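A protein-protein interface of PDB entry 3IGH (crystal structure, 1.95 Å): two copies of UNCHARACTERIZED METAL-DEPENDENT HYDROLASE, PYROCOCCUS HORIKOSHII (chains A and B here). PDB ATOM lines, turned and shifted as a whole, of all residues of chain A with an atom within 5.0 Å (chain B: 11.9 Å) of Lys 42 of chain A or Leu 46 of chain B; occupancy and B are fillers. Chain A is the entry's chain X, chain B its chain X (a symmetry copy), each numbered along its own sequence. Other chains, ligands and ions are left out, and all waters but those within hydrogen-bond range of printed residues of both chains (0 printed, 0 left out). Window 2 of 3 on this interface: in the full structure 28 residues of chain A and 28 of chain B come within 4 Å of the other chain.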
ATOM      1  N   TYR A  33      17.223 -15.388  34.139  1.00  0.00           N
ATOM      2  CA  TYR A  33      18.458 -15.886  34.715  1.00  0.00           C
ATOM      3  C   TYR A  33      18.263 -16.121  36.215  1.00  0.00           C
ATOM      4  O   TYR A  33      17.656 -15.305  36.902  1.00  0.00           O
ATOM      5  CB  TYR A  33      19.624 -14.913  34.456  1.00  0.00           C
ATOM      6  CG  TYR A  33      20.924 -15.332  35.116  1.00  0.00           C
ATOM      7  CD1 TYR A  33      21.722 -16.332  34.556  1.00  0.00           C
ATOM      8  CD2 TYR A  33      21.348 -14.737  36.305  1.00  0.00           C
ATOM      9  CE1 TYR A  33      22.907 -16.730  35.167  1.00  0.00           C
ATOM     10  CE2 TYR A  33      22.529 -15.124  36.920  1.00  0.00           C
ATOM     11  CZ  TYR A  33      23.301 -16.121  36.350  1.00  0.00           C
ATOM     12  OH  TYR A  33      24.471 -16.504  36.965  1.00  0.00           O
ATOM     13  N   GLU A  38      26.389 -11.325  41.052  1.00  0.00           N
ATOM     14  CA  GLU A  38      27.209 -10.422  40.234  1.00  0.00           C
ATOM     15  C   GLU A  38      26.893 -10.527  38.741  1.00  0.00           C
ATOM     16  O   GLU A  38      26.887  -9.515  38.034  1.00  0.00           O
ATOM     17  CB  GLU A  38      28.709 -10.647  40.481  1.00  0.00           C
ATOM     18  CG  GLU A  38      29.252  -9.956  41.735  1.00  0.00           C
ATOM     19  CD  GLU A  38      29.129  -8.436  41.677  1.00  0.00           C
ATOM     20  OE1 GLU A  38      28.483  -7.858  42.577  1.00  0.00           O
ATOM     21  OE2 GLU A  38      29.669  -7.823  40.731  1.00  0.00           O
ATOM     22  N   VAL A  39      26.635 -11.750  38.280  1.00  0.00           N
ATOM     23  CA  VAL A  39      26.237 -12.006  36.891  1.00  0.00           C
ATOM     24  C   VAL A  39      24.882 -11.352  36.580  1.00  0.00           C
ATOM     25  O   VAL A  39      24.720 -10.705  35.542  1.00  0.00           O
ATOM     26  CB  VAL A  39      26.200 -13.523  36.588  1.00  0.00           C
ATOM     27  CG1 VAL A  39      25.816 -13.786  35.136  1.00  0.00           C
ATOM     28  CG2 VAL A  39      27.549 -14.152  36.893  1.00  0.00           C
ATOM     29  N   ALA A  40      23.935 -11.501  37.505  1.00  0.00           N
ATOM     30  CA  ALA A  40      22.607 -10.902  37.387  1.00  0.00           C
ATOM     31  C   ALA A  40      22.673  -9.383  37.249  1.00  0.00           C
ATOM     32  O   ALA A  40      22.024  -8.813  36.372  1.00  0.00           O
ATOM     33  CB  ALA A  40      21.726 -11.296  38.584  1.00  0.00           C
ATOM     34  N   LYS A  41      23.476  -8.747  38.104  1.00  0.00           N
ATOM     35  CA  LYS A  41      23.665  -7.293  38.096  1.00  0.00           C
ATOM     36  C   LYS A  41      24.315  -6.821  36.795  1.00  0.00           C
ATOM     37  O   LYS A  41      23.948  -5.777  36.257  1.00  0.00           O
ATOM     38  CB  LYS A  41      24.495  -6.856  39.317  1.00  0.00           C
ATOM     39  CG  LYS A  41      24.683  -5.337  39.474  1.00  0.00           C
ATOM     40  CD  LYS A  41      25.121  -4.934  40.887  1.00  0.00           C
ATOM     41  CE  LYS A  41      26.552  -5.363  41.221  1.00  0.00           C
ATOM     42  NZ  LYS A  41      27.584  -4.464  40.628  1.00  0.00           N
ATOM     43  N   LYS A  42      25.256  -7.617  36.288  1.00  0.00           N
ATOM     44  CA  LYS A  42      25.983  -7.316  35.057  1.00  0.00           C
ATOM     45  C   LYS A  42      25.060  -7.322  33.840  1.00  0.00           C
ATOM     46  O   LYS A  42      25.142  -6.427  32.994  1.00  0.00           O
ATOM     47  CB  LYS A  42      27.120  -8.323  34.858  1.00  0.00           C
ATOM     48  CG  LYS A  42      28.122  -7.936  33.779  1.00  0.00           C
ATOM     49  CD  LYS A  42      29.311  -8.893  33.741  1.00  0.00           C
ATOM     50  CE  LYS A  42      30.263  -8.676  34.918  1.00  0.00           C
ATOM     51  NZ  LYS A  42      31.469  -9.545  34.827  1.00  0.00           N
ATOM     52  N   ILE A  43      24.189  -8.331  33.770  1.00  0.00           N
ATOM     53  CA  ILE A  43      23.194  -8.462  32.703  1.00  0.00           C
ATOM     54  C   ILE A  43      22.318  -7.207  32.615  1.00  0.00           C
ATOM     55  O   ILE A  43      22.166  -6.619  31.542  1.00  0.00           O
ATOM     56  CB  ILE A  43      22.332  -9.754  32.887  1.00  0.00           C
ATOM     57  CG1 ILE A  43      23.171 -11.003  32.597  1.00  0.00           C
ATOM     58  CG2 ILE A  43      21.107  -9.751  31.972  1.00  0.00           C
ATOM     59  CD1 ILE A  43      22.624 -12.276  33.228  1.00  0.00           C
ATOM     60  N   VAL A  44      21.794  -6.777  33.760  1.00  0.00           N
ATOM     61  CA  VAL A  44      20.876  -5.640  33.829  1.00  0.00           C
ATOM     62  C   VAL A  44      21.594  -4.294  33.648  1.00  0.00           C
ATOM     63  O   VAL A  44      20.979  -3.304  33.236  1.00  0.00           O
ATOM     64  CB  VAL A  44      20.005  -5.705  35.113  1.00  0.00           C
ATOM     65  CG1 VAL A  44      19.122  -4.480  35.275  1.00  0.00           C
ATOM     66  CG2 VAL A  44      19.122  -6.943  35.056  1.00  0.00           C
ATOM     67  N   GLU A  45      22.895  -4.268  33.928  1.00  0.00           N
ATOM     68  CA  GLU A  45      23.711  -3.082  33.654  1.00  0.00           C
ATOM     69  C   GLU A  45      23.899  -2.862  32.154  1.00  0.00           C
ATOM     70  O   GLU A  45      23.782  -1.735  31.671  1.00  0.00           O
ATOM     71  CB  GLU A  45      25.059  -3.160  34.377  1.00  0.00           C
ATOM     72  CG  GLU A  45      24.999  -2.594  35.790  1.00  0.00           C
ATOM     73  CD  GLU A  45      26.172  -3.004  36.667  1.00  0.00           C
ATOM     74  OE1 GLU A  45      27.006  -3.832  36.232  1.00  0.00           O
ATOM     75  OE2 GLU A  45      26.250  -2.493  37.806  1.00  0.00           O
ATOM     76  N   LEU A  46      24.162  -3.950  31.430  1.00  0.00           N
ATOM     77  CA  LEU A  46      24.328  -3.920  29.979  1.00  0.00           C
ATOM     78  C   LEU A  46      23.020  -3.599  29.261  1.00  0.00           C
ATOM     79  O   LEU A  46      22.999  -2.780  28.339  1.00  0.00           O
ATOM     80  CB  LEU A  46      24.876  -5.258  29.470  1.00  0.00           C
ATOM     81  CG  LEU A  46      26.296  -5.693  29.842  1.00  0.00           C
ATOM     82  CD1 LEU A  46      26.476  -7.179  29.557  1.00  0.00           C
ATOM     83  CD2 LEU A  46      27.355  -4.866  29.105  1.00  0.00           C
ATOM     84  N   SER B   2      13.383 -19.438  25.467  1.00  0.00           N
ATOM     85  CA  SER B   2      14.828 -19.299  25.112  1.00  0.00           C
ATOM     86  C   SER B   2      15.260 -17.835  25.078  1.00  0.00           C
ATOM     87  O   SER B   2      14.459 -16.951  24.754  1.00  0.00           O
ATOM     88  CB  SER B   2      15.111 -19.946  23.752  1.00  0.00           C
ATOM     89  OG  SER B   2      14.923 -21.348  23.799  1.00  0.00           O
ATOM     90  N   LEU B   3      16.525 -17.585  25.420  1.00  0.00           N
ATOM     91  CA  LEU B   3      17.112 -16.260  25.258  1.00  0.00           C
ATOM     92  C   LEU B   3      18.039 -16.275  24.058  1.00  0.00           C
ATOM     93  O   LEU B   3      19.028 -17.007  24.052  1.00  0.00           O
ATOM     94  CB  LEU B   3      17.901 -15.837  26.497  1.00  0.00           C
ATOM     95  CG  LEU B   3      17.712 -14.357  26.829  1.00  0.00           C
ATOM     96  CD1 LEU B   3      16.837 -14.238  28.045  1.00  0.00           C
ATOM     97  CD2 LEU B   3      19.016 -13.658  27.088  1.00  0.00           C
ATOM     98  N   LYS B   4      17.755 -15.463  23.051  1.00  0.00           N
ATOM     99  CA  LYS B   4      18.617 -15.412  21.891  1.00  0.00           C
ATOM    100  C   LYS B   4      19.072 -14.040  21.465  1.00  0.00           C
ATOM    101  O   LYS B   4      18.422 -13.066  21.736  1.00  0.00           O
ATOM    102  CB  LYS B   4      18.022 -16.181  20.738  1.00  0.00           C
ATOM    103  CG  LYS B   4      16.882 -15.526  20.091  1.00  0.00           C
ATOM    104  CD  LYS B   4      16.460 -16.242  18.824  1.00  0.00           C
ATOM    105  CE  LYS B   4      14.958 -16.477  18.828  1.00  0.00           C
ATOM    106  NZ  LYS B   4      14.219 -16.058  17.600  1.00  0.00           N
ATOM    107  N   ALA B   5      20.212 -13.978  20.809  1.00  0.00           N
ATOM    108  CA  ALA B   5      20.699 -12.743  20.212  1.00  0.00           C
ATOM    109  C   ALA B   5      20.728 -12.844  18.691  1.00  0.00           C
ATOM    110  O   ALA B   5      21.089 -13.882  18.135  1.00  0.00           O
ATOM    111  CB  ALA B   5      22.073 -12.373  20.753  1.00  0.00           C
ATOM    112  N   ILE B   7      22.718 -10.939  15.929  1.00  0.00           N
ATOM    113  CA  ILE B   7      23.905 -10.077  15.889  1.00  0.00           C
ATOM    114  C   ILE B   7      24.507 -10.010  14.485  1.00  0.00           C
ATOM    115  O   ILE B   7      24.177 -10.838  13.627  1.00  0.00           O
ATOM    116  CB  ILE B   7      25.015 -10.560  16.876  1.00  0.00           C
ATOM    117  CG1 ILE B   7      25.521 -11.960  16.500  1.00  0.00           C
ATOM    118  CG2 ILE B   7      24.534 -10.501  18.332  1.00  0.00           C
ATOM    119  CD1 ILE B   7      26.990 -12.174  16.774  1.00  0.00           C
ATOM    120  N   VAL B  25      18.331  -8.563  21.441  1.00  0.00           N
ATOM    121  CA  VAL B  25      18.179  -9.687  22.368  1.00  0.00           C
ATOM    122  C   VAL B  25      16.701  -9.993  22.529  1.00  0.00           C
ATOM    123  O   VAL B  25      15.906  -9.093  22.792  1.00  0.00           O
ATOM    124  CB  VAL B  25      18.819  -9.428  23.756  1.00  0.00           C
ATOM    125  CG1 VAL B  25      18.726 -10.677  24.621  1.00  0.00           C
ATOM    126  CG2 VAL B  25      20.274  -9.029  23.609  1.00  0.00           C
ATOM    127  N   ILE B  32      14.188  -7.459  24.270  1.00  0.00           N
ATOM    128  CA  ILE B  32      14.577  -6.882  25.571  1.00  0.00           C
ATOM    129  C   ILE B  32      15.778  -5.940  25.508  1.00  0.00           C
ATOM    130  O   ILE B  32      15.994  -5.118  26.408  1.00  0.00           O
ATOM    131  CB  ILE B  32      14.751  -7.964  26.657  1.00  0.00           C
ATOM    132  CG1 ILE B  32      15.802  -8.995  26.255  1.00  0.00           C
ATOM    133  CG2 ILE B  32      13.423  -8.655  26.916  1.00  0.00           C
ATOM    134  CD1 ILE B  32      16.363  -9.769  27.431  1.00  0.00           C
ATOM    135  N   TYR B  33      16.548  -6.061  24.430  1.00  0.00           N
ATOM    136  CA  TYR B  33      17.613  -5.127  24.113  1.00  0.00           C
ATOM    137  C   TYR B  33      17.674  -4.916  22.598  1.00  0.00           C
ATOM    138  O   TYR B  33      17.567  -5.868  21.831  1.00  0.00           O
ATOM    139  CB  TYR B  33      18.967  -5.621  24.657  1.00  0.00           C
ATOM    140  CG  TYR B  33      20.136  -4.733  24.276  1.00  0.00           C
ATOM    141  CD1 TYR B  33      20.377  -3.536  24.953  1.00  0.00           C
ATOM    142  CD2 TYR B  33      20.993  -5.085  23.232  1.00  0.00           C
ATOM    143  CE1 TYR B  33      21.439  -2.712  24.597  1.00  0.00           C
ATOM    144  CE2 TYR B  33      22.056  -4.272  22.870  1.00  0.00           C
ATOM    145  CZ  TYR B  33      22.272  -3.087  23.552  1.00  0.00           C
ATOM    146  OH  TYR B  33      23.327  -2.282  23.189  1.00  0.00           O
ATOM    147  N   SER B  37      25.745  -4.743  18.545  1.00  0.00           N
ATOM    148  CA  SER B  37      25.895  -6.177  18.321  1.00  0.00           C
ATOM    149  C   SER B  37      26.745  -6.892  19.383  1.00  0.00           C
ATOM    150  O   SER B  37      26.419  -8.013  19.789  1.00  0.00           O
ATOM    151  CB  SER B  37      26.480  -6.402  16.923  1.00  0.00           C
ATOM    152  OG  SER B  37      26.669  -7.774  16.647  1.00  0.00           O
ATOM    153  N   GLU B  38      27.822  -6.244  19.826  1.00  0.00           N
ATOM    154  CA  GLU B  38      28.717  -6.821  20.838  1.00  0.00           C
ATOM    155  C   GLU B  38      28.071  -6.898  22.221  1.00  0.00           C
ATOM    156  O   GLU B  38      28.279  -7.872  22.952  1.00  0.00           O
ATOM    157  CB  GLU B  38      30.049  -6.058  20.910  1.00  0.00           C
ATOM    158  CG  GLU B  38      31.062  -6.454  19.832  1.00  0.00           C
ATOM    159  CD  GLU B  38      31.488  -7.916  19.924  1.00  0.00           C
ATOM    160  OE1 GLU B  38      31.305  -8.651  18.931  1.00  0.00           O
ATOM    161  OE2 GLU B  38      31.995  -8.331  20.989  1.00  0.00           O
ATOM    162  N   VAL B  39      27.294  -5.872  22.566  1.00  0.00           N
ATOM    163  CA  VAL B  39      26.541  -5.834  23.825  1.00  0.00           C
ATOM    164  C   VAL B  39      25.482  -6.947  23.863  1.00  0.00           C
ATOM    165  O   VAL B  39      25.346  -7.651  24.867  1.00  0.00           O
ATOM    166  CB  VAL B  39      25.894  -4.448  24.051  1.00  0.00           C
ATOM    167  CG1 VAL B  39      25.137  -4.401  25.373  1.00  0.00           C
ATOM    168  CG2 VAL B  39      26.955  -3.361  24.018  1.00  0.00           C
ATOM    169  N   ALA B  40      24.769  -7.113  22.750  1.00  0.00           N
ATOM    170  CA  ALA B  40      23.756  -8.157  22.604  1.00  0.00           C
ATOM    171  C   ALA B  40      24.336  -9.553  22.815  1.00  0.00           C
ATOM    172  O   ALA B  40      23.765 -10.355  23.554  1.00  0.00           O
ATOM    173  CB  ALA B  40      23.072  -8.059  21.231  1.00  0.00           C
ATOM    174  N   LYS B  41      25.478  -9.820  22.180  1.00  0.00           N
ATOM    175  CA  LYS B  41      26.175 -11.105  22.288  1.00  0.00           C
ATOM    176  C   LYS B  41      26.655 -11.362  23.717  1.00  0.00           C
ATOM    177  O   LYS B  41      26.584 -12.490  24.205  1.00  0.00           O
ATOM    178  CB  LYS B  41      27.348 -11.162  21.293  1.00  0.00           C
ATOM    179  CG  LYS B  41      28.103 -12.502  21.242  1.00  0.00           C
ATOM    180  CD  LYS B  41      28.951 -12.661  19.975  1.00  0.00           C
ATOM    181  CE  LYS B  41      30.165 -11.729  19.940  1.00  0.00           C
ATOM    182  NZ  LYS B  41      31.299 -12.217  20.777  1.00  0.00           N
ATOM    183  N   LYS B  42      27.111 -10.302  24.381  1.00  0.00           N
ATOM    184  CA  LYS B  42      27.614 -10.369  25.751  1.00  0.00           C
ATOM    185  C   LYS B  42      26.512 -10.748  26.740  1.00  0.00           C
ATOM    186  O   LYS B  42      26.729 -11.586  27.620  1.00  0.00           O
ATOM    187  CB  LYS B  42      28.238  -9.028  26.150  1.00  0.00           C
ATOM    188  CG  LYS B  42      29.054  -9.070  27.433  1.00  0.00           C
ATOM    189  CD  LYS B  42      29.778  -7.749  27.688  1.00  0.00           C
ATOM    190  CE  LYS B  42      30.973  -7.559  26.754  1.00  0.00           C
ATOM    191  NZ  LYS B  42      31.732  -6.317  27.067  1.00  0.00           N
ATOM    192  N   ILE B  43      25.342 -10.126  26.579  1.00  0.00           N
ATOM    193  CA  ILE B  43      24.162 -10.408  27.401  1.00  0.00           C
ATOM    194  C   ILE B  43      23.803 -11.898  27.349  1.00  0.00           C
ATOM    195  O   ILE B  43      23.648 -12.544  28.387  1.00  0.00           O
ATOM    196  CB  ILE B  43      22.953  -9.509  26.982  1.00  0.00           C
ATOM    197  CG1 ILE B  43      23.198  -8.054  27.395  1.00  0.00           C
ATOM    198  CG2 ILE B  43      21.645  -9.993  27.611  1.00  0.00           C
ATOM    199  CD1 ILE B  43      22.378  -7.041  26.609  1.00  0.00           C
ATOM    200  N   VAL B  44      23.730 -12.441  26.136  1.00  0.00           N
ATOM    201  CA  VAL B  44      23.325 -13.829  25.918  1.00  0.00           C
ATOM    202  C   VAL B  44      24.424 -14.830  26.304  1.00  0.00           C
ATOM    203  O   VAL B  44      24.136 -15.991  26.615  1.00  0.00           O
ATOM    204  CB  VAL B  44      22.788 -14.032  24.475  1.00  0.00           C
ATOM    205  CG1 VAL B  44      22.465 -15.485  24.177  1.00  0.00           C
ATOM    206  CG2 VAL B  44      21.526 -13.201  24.290  1.00  0.00           C
ATOM    207  N   GLU B  45      25.674 -14.371  26.312  1.00  0.00           N
ATOM    208  CA  GLU B  45      26.784 -15.192  26.804  1.00  0.00           C
ATOM    209  C   GLU B  45      26.711 -15.390  28.317  1.00  0.00           C
ATOM    210  O   GLU B  45      26.909 -16.502  28.809  1.00  0.00           O
ATOM    211  CB  GLU B  45      28.134 -14.602  26.385  1.00  0.00           C
ATOM    212  CG  GLU B  45      28.589 -15.093  25.017  1.00  0.00           C
ATOM    213  CD  GLU B  45      29.693 -14.251  24.398  1.00  0.00           C
ATOM    214  OE1 GLU B  45      30.057 -13.195  24.968  1.00  0.00           O
ATOM    215  OE2 GLU B  45      30.194 -14.651  23.324  1.00  0.00           O
ATOM    216  N   LEU B  46      26.400 -14.311  29.035  1.00  0.00           N
ATOM    217  CA  LEU B  46      26.249 -14.339  30.488  1.00  0.00           C
ATOM    218  C   LEU B  46      25.024 -15.140  30.920  1.00  0.00           C
ATOM    219  O   LEU B  46      25.102 -15.949  31.849  1.00  0.00           O
ATOM    220  CB  LEU B  46      26.151 -12.915  31.048  1.00  0.00           C
ATOM    221  CG  LEU B  46      27.362 -11.980  30.974  1.00  0.00           C
ATOM    222  CD1 LEU B  46      26.926 -10.543  31.230  1.00  0.00           C
ATOM    223  CD2 LEU B  46      28.463 -12.398  31.954  1.00  0.00           C
ATOM    224  N   SER B  47      23.905 -14.910  30.232  1.00  0.00           N
ATOM    225  CA  SER B  47      22.633 -15.561  30.543  1.00  0.00           C
ATOM    226  C   SER B  47      22.611 -17.018  30.109  1.00  0.00           C
ATOM    227  O   SER B  47      21.943 -17.846  30.725  1.00  0.00           O
ATOM    228  CB  SER B  47      21.473 -14.830  29.861  1.00  0.00           C
ATOM    229  OG  SER B  47      21.111 -13.655  30.558  1.00  0.00           O
ATOM    230  N   GLY B  48      23.328 -17.317  29.029  1.00  0.00           N
ATOM    231  CA  GLY B  48      23.239 -18.626  28.391  1.00  0.00           C
ATOM    232  C   GLY B  48      22.133 -18.567  27.350  1.00  0.00           C
ATOM    233  O   GLY B  48      21.051 -18.026  27.603  1.00  0.00           O
ATOM    234  N   GLY B  49      22.403 -19.109  26.169  1.00  0.00           N
ATOM    235  CA  GLY B  49      21.421 -19.107  25.091  1.00  0.00           C
ATOM    236  C   GLY B  49      22.033 -19.059  23.705  1.00  0.00           C
ATOM    237  O   GLY B  49      23.256 -19.062  23.549  1.00  0.00           O
ATOM    238  N   GLU B  50      21.167 -19.000  22.698  1.00  0.00           N
ATOM    239  CA  GLU B  50      21.574 -19.074  21.298  1.00  0.00           C
ATOM    240  C   GLU B  50      22.034 -17.716  20.772  1.00  0.00           C
ATOM    241  O   GLU B  50      21.398 -16.692  21.022  1.00  0.00           O
ATOM    242  CB  GLU B  50      20.410 -19.609  20.459  1.00  0.00           C
ATOM    243  CG  GLU B  50      20.755 -19.997  19.027  1.00  0.00           C
ATOM    244  CD  GLU B  50      19.528 -20.387  18.209  1.00  0.00           C
ATOM    245  OE1 GLU B  50      18.385 -20.141  18.660  1.00  0.00           O
ATOM    246  OE2 GLU B  50      19.707 -20.939  17.102  1.00  0.00           O
ATOM    247  N   ILE B  51      23.151 -17.708  20.055  1.00  0.00           N
ATOM    248  CA  ILE B  51      23.608 -16.499  19.379  1.00  0.00           C
ATOM    249  C   ILE B  51      23.528 -16.724  17.872  1.00  0.00           C
ATOM    250  O   ILE B  51      24.226 -17.575  17.321  1.00  0.00           O
ATOM    251  CB  ILE B  51      25.028 -16.076  19.827  1.00  0.00           C
ATOM    252  CG1 ILE B  51      25.048 -15.798  21.335  1.00  0.00           C
ATOM    253  CG2 ILE B  51      25.488 -14.841  19.060  1.00  0.00           C
ATOM    254  CD1 ILE B  51      26.421 -15.863  21.967  1.00  0.00           C
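Among the printed residues, merely in contact across the chains: Val 39 of chain A with Leu 46 of chain B (3.999 Å), Lys 42 of chain A with Leu 46 of chain B (3.8 Å), Ile 43 of chain A with Leu 46 of chain B (3.9 Å), Ile 43 of chain A with Ser 47 of chain B (3.4 Å), Leu 46 of chain A with Val 39 of chain B (3.999 Å), Leu 46 of chain A with Lys 42 of chain B (3.8 Å), Leu 46 of chain A with Ile 43 of chain B (3.9 Å) and Leu 46 of chain A with Leu 46 of chain B (3.8 Å).
Printed residues of chain B within 4 Å of Val 39 of chain A: Leu 46.
No residue of chain B comes within 4 Å of Ala 40 of chain A.
No residue of chain B comes within 4 Å of Lys 41 of chain A.
Of chain B, only Leu 46 comes within 4 Å of Lys 42 of chain A.
Printed residues of chain B within 4 Å of Ile 43 of chain A: Leu 46 and Ser 47.
No residue of chain B comes within 4 Å of Glu 45 of chain A.
Printed residues of chain B within 4 Å of Leu 46 of chain A: Val 39 (3.999 Å), Lys 42 (3.8 Å), Ile 43 (3.9 Å) and Leu 46 (3.8 Å).
Of the printed residues of chain A, Lys 42 of chain B touches Leu 46 (3.8 Å).
Of the printed residues of chain A, Ile 43 of chain B touches Leu 46 (3.9 Å).
The nearest residue of chain B that does not touch Lys 42 of chain A is Ile 43 of chain B (6.1 Å).
The nearest printed residue of chain A that does not touch Leu 46 of chain B is Tyr 33 of chain A (4.1 Å).
Hydrophobic or aromatic side chains of chain B that line the printed part of chain A: Val 39, Ile 43 and Leu 46.
Of the 10 printed residues of chain A, 4 touch a printed residue of chain B.
Among the printed residues, no Asp or Glu carboxylate lies within 4 Å of a Lys or Arg side-chain nitrogen of the other chain.
Val 39 of chain A touches Leu 46 of chain B, and with the chains exchanged Leu 46 of chain A touches Val 39 of chain B.
Lys 42 of chain A touches Leu 46 of chain B, and with the chains exchanged Leu 46 of chain A touches Lys 42 of chain B.
Ile 43 of chain A touches Leu 46 of chain B, and with the chains exchanged Leu 46 of chain A touches Ile 43 of chain B.
Leu 46 of chain B touches its own counterpart, Leu 46 of chain A.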
